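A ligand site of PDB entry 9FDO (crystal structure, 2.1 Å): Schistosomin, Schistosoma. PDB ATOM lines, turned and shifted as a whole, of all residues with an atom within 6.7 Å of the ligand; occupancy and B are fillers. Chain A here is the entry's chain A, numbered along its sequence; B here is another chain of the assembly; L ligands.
The backbone carbonyl oxygen of Glu 13 lies within hydrogen-bond range of a nitrogen (N1) of the ligand (3.0 Å).
A carbon (C1) of the ligand is covalently linked to the side-chain amino group (NZ) of Lys 80 of chain B.
NZ of Lys 41 is in hydrogen-bond range of O2 of the ligand (2.8 Å).
O2 of the ligand lies close to SG of Cys 14.
Merely in contact with the ligand: Arg 4, Phe 44, Tyr 3, Cys 45 and Phe 12.
Hydrophobic or aromatic side chains within 4 Å of the ligand: Tyr 3, Phe 12 and Phe 44.
Of the 18 residues printed, 9 come within 4 Å of the ligand.
The side-chain sulfur of Cys 45 forms a disulfide with the side-chain sulfur of Cys 5, 2.0 Å away.
The side-chain sulfur (SG) of Cys 14 forms a disulfide with the side-chain sulfur (SG) of Cys 38, 2.0 Å away.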
ATOM      1  N   TYR A   3      31.427  22.891 -14.138  1.00  0.00           N
ATOM      2  CA  TYR A   3      30.827  23.443 -15.344  1.00  0.00           C
ATOM      3  C   TYR A   3      30.353  24.872 -15.064  1.00  0.00           C
ATOM      4  O   TYR A   3      29.608  25.106 -14.122  1.00  0.00           O
ATOM      5  CB  TYR A   3      29.730  22.525 -15.865  1.00  0.00           C
ATOM      6  CG  TYR A   3      29.616  22.461 -17.375  1.00  0.00           C
ATOM      7  CD1 TYR A   3      30.156  23.462 -18.180  1.00  0.00           C
ATOM      8  CD2 TYR A   3      28.897  21.453 -17.994  1.00  0.00           C
ATOM      9  CE1 TYR A   3      30.006  23.440 -19.560  1.00  0.00           C
ATOM     10  CE2 TYR A   3      28.726  21.425 -19.371  1.00  0.00           C
ATOM     11  CZ  TYR A   3      29.284  22.421 -20.160  1.00  0.00           C
ATOM     12  OH  TYR A   3      29.119  22.409 -21.527  1.00  0.00           O
ATOM     13  N   ARG A   4      30.859  25.842 -15.841  1.00  0.00           N
ATOM     14  CA  ARG A   4      30.637  27.264 -15.611  1.00  0.00           C
ATOM     15  C   ARG A   4      29.394  27.882 -16.215  1.00  0.00           C
ATOM     16  O   ARG A   4      28.902  27.421 -17.242  1.00  0.00           O
ATOM     17  CB  ARG A   4      31.866  28.063 -16.134  1.00  0.00           C
ATOM     18  CG  ARG A   4      32.878  28.466 -15.072  1.00  0.00           C
ATOM     19  CD  ARG A   4      34.175  28.878 -15.723  1.00  0.00           C
ATOM     20  NE  ARG A   4      35.336  28.330 -15.002  1.00  0.00           N
ATOM     21  CZ  ARG A   4      36.567  28.266 -15.507  1.00  0.00           C
ATOM     22  NH1 ARG A   4      36.818  28.693 -16.740  1.00  0.00           N
ATOM     23  NH2 ARG A   4      37.554  27.751 -14.786  1.00  0.00           N
ATOM     24  N   CYS A   5      28.948  28.986 -15.618  1.00  0.00           N
ATOM     25  CA  CYS A   5      27.871  29.828 -16.129  1.00  0.00           C
ATOM     26  C   CYS A   5      28.417  30.497 -17.372  1.00  0.00           C
ATOM     27  O   CYS A   5      29.602  30.872 -17.403  1.00  0.00           O
ATOM     28  CB  CYS A   5      27.478  30.872 -15.074  1.00  0.00           C
ATOM     29  SG  CYS A   5      26.477  30.225 -13.717  1.00  0.00           S
ATOM     30  N   PRO A   6      27.608  30.625 -18.441  1.00  0.00           N
ATOM     31  CA  PRO A   6      28.133  31.285 -19.657  1.00  0.00           C
ATOM     32  C   PRO A   6      28.362  32.778 -19.449  1.00  0.00           C
ATOM     33  O   PRO A   6      27.742  33.406 -18.582  1.00  0.00           O
ATOM     34  CB  PRO A   6      27.048  30.993 -20.707  1.00  0.00           C
ATOM     35  CG  PRO A   6      25.842  30.736 -19.964  1.00  0.00           C
ATOM     36  CD  PRO A   6      26.207  30.213 -18.602  1.00  0.00           C
ATOM     37  N   ALA A  11      25.859  31.378 -25.530  1.00  0.00           N
ATOM     38  CA  ALA A  11      24.674  30.542 -25.569  1.00  0.00           C
ATOM     39  C   ALA A  11      24.463  29.766 -24.273  1.00  0.00           C
ATOM     40  O   ALA A  11      25.428  29.238 -23.690  1.00  0.00           O
ATOM     41  CB  ALA A  11      24.793  29.547 -26.720  1.00  0.00           C
ATOM     42  N   PHE A  12      23.226  29.717 -23.805  1.00  0.00           N
ATOM     43  CA  PHE A  12      22.911  28.911 -22.630  1.00  0.00           C
ATOM     44  C   PHE A  12      22.507  27.578 -23.220  1.00  0.00           C
ATOM     45  O   PHE A  12      21.469  27.456 -23.850  1.00  0.00           O
ATOM     46  CB  PHE A  12      21.781  29.522 -21.808  1.00  0.00           C
ATOM     47  CG  PHE A  12      21.629  28.821 -20.473  1.00  0.00           C
ATOM     48  CD1 PHE A  12      20.915  27.630 -20.380  1.00  0.00           C
ATOM     49  CD2 PHE A  12      22.159  29.366 -19.310  1.00  0.00           C
ATOM     50  CE1 PHE A  12      20.771  26.990 -19.159  1.00  0.00           C
ATOM     51  CE2 PHE A  12      21.994  28.734 -18.088  1.00  0.00           C
ATOM     52  CZ  PHE A  12      21.325  27.538 -18.017  1.00  0.00           C
ATOM     53  N   GLU A  13      23.419  26.620 -23.159  1.00  0.00           N
ATOM     54  CA  GLU A  13      23.196  25.326 -23.747  1.00  0.00           C
ATOM     55  C   GLU A  13      23.184  24.315 -22.641  1.00  0.00           C
ATOM     56  O   GLU A  13      24.184  24.096 -21.952  1.00  0.00           O
ATOM     57  CB  GLU A  13      24.256  25.030 -24.809  1.00  0.00           C
ATOM     58  CG  GLU A  13      24.149  26.010 -25.949  1.00  0.00           C
ATOM     59  CD  GLU A  13      25.108  25.803 -27.101  1.00  0.00           C
ATOM     60  OE1 GLU A  13      24.803  26.313 -28.213  1.00  0.00           O
ATOM     61  OE2 GLU A  13      26.147  25.129 -26.897  1.00  0.00           O
ATOM     62  N   CYS A  14      22.015  23.745 -22.441  1.00  0.00           N
ATOM     63  CA  CYS A  14      21.804  22.818 -21.377  1.00  0.00           C
ATOM     64  C   CYS A  14      20.978  21.620 -21.854  1.00  0.00           C
ATOM     65  O   CYS A  14      19.938  21.815 -22.481  1.00  0.00           O
ATOM     66  CB  CYS A  14      21.126  23.561 -20.230  1.00  0.00           C
ATOM     67  SG  CYS A  14      20.625  22.524 -18.861  1.00  0.00           S
ATOM     68  N   PHE A  15      21.440  20.401 -21.564  1.00  0.00           N
ATOM     69  CA  PHE A  15      20.698  19.190 -21.882  1.00  0.00           C
ATOM     70  C   PHE A  15      19.765  18.877 -20.708  1.00  0.00           C
ATOM     71  O   PHE A  15      20.231  18.643 -19.594  1.00  0.00           O
ATOM     72  CB  PHE A  15      21.646  18.007 -22.076  1.00  0.00           C
ATOM     73  CG  PHE A  15      22.638  18.191 -23.190  1.00  0.00           C
ATOM     74  CD1 PHE A  15      22.266  18.775 -24.390  1.00  0.00           C
ATOM     75  CD2 PHE A  15      23.942  17.736 -23.057  1.00  0.00           C
ATOM     76  CE1 PHE A  15      23.166  18.870 -25.446  1.00  0.00           C
ATOM     77  CE2 PHE A  15      24.846  17.839 -24.108  1.00  0.00           C
ATOM     78  CZ  PHE A  15      24.455  18.410 -25.298  1.00  0.00           C
ATOM     79  N   CYS A  38      17.369  22.722 -16.174  1.00  0.00           N
ATOM     80  CA  CYS A  38      18.001  23.774 -16.959  1.00  0.00           C
ATOM     81  C   CYS A  38      17.588  25.148 -16.464  1.00  0.00           C
ATOM     82  O   CYS A  38      18.431  26.051 -16.412  1.00  0.00           O
ATOM     83  CB  CYS A  38      17.757  23.593 -18.461  1.00  0.00           C
ATOM     84  SG  CYS A  38      18.644  22.179 -19.187  1.00  0.00           S
ATOM     85  N   ARG A  40      16.711  25.789 -13.308  1.00  0.00           N
ATOM     86  CA  ARG A  40      17.353  25.849 -12.019  1.00  0.00           C
ATOM     87  C   ARG A  40      18.786  26.339 -12.185  1.00  0.00           C
ATOM     88  O   ARG A  40      19.197  27.224 -11.440  1.00  0.00           O
ATOM     89  CB  ARG A  40      17.314  24.465 -11.346  1.00  0.00           C
ATOM     90  CG  ARG A  40      17.957  24.452  -9.969  1.00  0.00           C
ATOM     91  CD  ARG A  40      18.467  23.081  -9.688  1.00  0.00           C
ATOM     92  NE  ARG A  40      19.623  23.087  -8.805  1.00  0.00           N
ATOM     93  CZ  ARG A  40      19.934  22.082  -7.982  1.00  0.00           C
ATOM     94  NH1 ARG A  40      19.162  20.995  -7.916  1.00  0.00           N
ATOM     95  NH2 ARG A  40      20.995  22.169  -7.200  1.00  0.00           N
ATOM     96  N   LYS A  41      19.512  25.864 -13.212  1.00  0.00           N
ATOM     97  CA  LYS A  41      20.868  26.332 -13.488  1.00  0.00           C
ATOM     98  C   LYS A  41      20.864  27.784 -14.008  1.00  0.00           C
ATOM     99  O   LYS A  41      21.762  28.565 -13.672  1.00  0.00           O
ATOM    100  CB  LYS A  41      21.558  25.451 -14.510  1.00  0.00           C
ATOM    101  CG  LYS A  41      21.813  24.030 -14.076  1.00  0.00           C
ATOM    102  CD  LYS A  41      22.232  23.222 -15.311  1.00  0.00           C
ATOM    103  CE  LYS A  41      22.121  21.754 -15.058  1.00  0.00           C
ATOM    104  NZ  LYS A  41      22.806  20.954 -16.105  1.00  0.00           N
ATOM    105  N   TYR A  42      19.844  28.129 -14.815  1.00  0.00           N
ATOM    106  CA  TYR A  42      19.677  29.478 -15.329  1.00  0.00           C
ATOM    107  C   TYR A  42      19.482  30.448 -14.170  1.00  0.00           C
ATOM    108  O   TYR A  42      20.090  31.509 -14.154  1.00  0.00           O
ATOM    109  CB  TYR A  42      18.473  29.596 -16.293  1.00  0.00           C
ATOM    110  CG  TYR A  42      18.365  31.004 -16.836  1.00  0.00           C
ATOM    111  CD1 TYR A  42      19.257  31.472 -17.798  1.00  0.00           C
ATOM    112  CD2 TYR A  42      17.456  31.901 -16.311  1.00  0.00           C
ATOM    113  CE1 TYR A  42      19.226  32.801 -18.232  1.00  0.00           C
ATOM    114  CE2 TYR A  42      17.404  33.224 -16.742  1.00  0.00           C
ATOM    115  CZ  TYR A  42      18.297  33.672 -17.695  1.00  0.00           C
ATOM    116  OH  TYR A  42      18.212  34.982 -18.124  1.00  0.00           O
ATOM    117  N   PHE A  44      20.488  30.166 -11.086  1.00  0.00           N
ATOM    118  CA  PHE A  44      21.753  30.311 -10.402  1.00  0.00           C
ATOM    119  C   PHE A  44      22.640  31.312 -11.153  1.00  0.00           C
ATOM    120  O   PHE A  44      23.243  32.176 -10.513  1.00  0.00           O
ATOM    121  CB  PHE A  44      22.474  28.962 -10.266  1.00  0.00           C
ATOM    122  CG  PHE A  44      23.799  29.111  -9.549  1.00  0.00           C
ATOM    123  CD1 PHE A  44      23.872  29.066  -8.153  1.00  0.00           C
ATOM    124  CD2 PHE A  44      24.978  29.340 -10.251  1.00  0.00           C
ATOM    125  CE1 PHE A  44      25.083  29.223  -7.493  1.00  0.00           C
ATOM    126  CE2 PHE A  44      26.188  29.483  -9.589  1.00  0.00           C
ATOM    127  CZ  PHE A  44      26.227  29.428  -8.215  1.00  0.00           C
ATOM    128  N   CYS A  45      22.742  31.214 -12.478  1.00  0.00           N
ATOM    129  CA  CYS A  45      23.604  32.094 -13.278  1.00  0.00           C
ATOM    130  C   CYS A  45      23.078  33.531 -13.418  1.00  0.00           C
ATOM    131  O   CYS A  45      23.879  34.470 -13.415  1.00  0.00           O
ATOM    132  CB  CYS A  45      23.880  31.470 -14.644  1.00  0.00           C
ATOM    133  SG  CYS A  45      24.663  29.837 -14.577  1.00  0.00           S
ATOM    134  N   ALA A  49      20.308  32.529  -7.646  1.00  0.00           N
ATOM    135  CA  ALA A  49      19.321  31.749  -6.918  1.00  0.00           C
ATOM    136  C   ALA A  49      19.802  30.330  -6.665  1.00  0.00           C
ATOM    137  O   ALA A  49      20.218  29.609  -7.570  1.00  0.00           O
ATOM    138  CB  ALA A  49      17.999  31.729  -7.679  1.00  0.00           C
ATOM    139  N   MET A  79      22.721  34.064 -22.745  1.00  0.00           N
ATOM    140  CA  MET A  79      22.940  34.689 -21.435  1.00  0.00           C
ATOM    141  C   MET A  79      23.154  36.194 -21.617  1.00  0.00           C
ATOM    142  O   MET A  79      23.888  36.613 -22.504  1.00  0.00           O
ATOM    143  CB  MET A  79      24.173  34.048 -20.752  1.00  0.00           C
ATOM    144  CG  MET A  79      24.447  34.591 -19.355  1.00  0.00           C
ATOM    145  SD  MET A  79      23.090  34.305 -18.170  1.00  0.00           S
ATOM    146  CE  MET A  79      22.921  32.576 -18.271  1.00  0.00           C
ATOM    147  N   LYS B  80      28.954  20.703  -7.701  1.00  0.00           N
ATOM    148  CA  LYS B  80      28.775  22.143  -7.716  1.00  0.00           C
ATOM    149  C   LYS B  80      29.725  22.837  -6.728  1.00  0.00           C
ATOM    150  O   LYS B  80      30.076  22.233  -5.712  1.00  0.00           O
ATOM    151  CB  LYS B  80      27.316  22.513  -7.453  1.00  0.00           C
ATOM    152  CG  LYS B  80      26.929  23.868  -8.012  1.00  0.00           C
ATOM    153  CD  LYS B  80      25.543  24.269  -7.575  1.00  0.00           C
ATOM    154  CE  LYS B  80      25.237  25.707  -7.908  1.00  0.00           C
ATOM    155  NZ  LYS B  80      25.285  25.981  -9.378  1.00  0.00           N
HETATM  156  C1  LIG L   1      24.635  25.610 -10.501  1.00  0.00           C
HETATM  157  O1  LIG L   1      23.452  25.664 -10.294  1.00  0.00           O
HETATM  158  C2  LIG L   1      25.213  25.105 -11.791  1.00  0.00           C
HETATM  159  C3  LIG L   1      25.968  26.158 -12.596  1.00  0.00           C
HETATM  160  C4  LIG L   1      25.524  26.287 -14.023  1.00  0.00           C
HETATM  161  C5  LIG L   1      26.017  25.175 -14.942  1.00  0.00           C
HETATM  162  C6  LIG L   1      26.262  25.615 -16.380  1.00  0.00           C
HETATM  163  S1  LIG L   1      24.837  26.446 -17.156  1.00  0.00           S
HETATM  164  C7  LIG L   1      25.507  26.161 -18.815  1.00  0.00           C
HETATM  165  C8  LIG L   1      26.219  24.799 -18.767  1.00  0.00           C
HETATM  166  N1  LIG L   1      25.338  23.714 -19.171  1.00  0.00           N
HETATM  167  C9  LIG L   1      25.074  22.859 -18.163  1.00  0.00           C
HETATM  168  O2  LIG L   1      24.317  21.893 -18.232  1.00  0.00           O
HETATM  169  N2  LIG L   1      25.766  23.245 -17.072  1.00  0.00           N
HETATM  170  C10 LIG L   1      26.573  24.422 -17.294  1.00  0.00           C
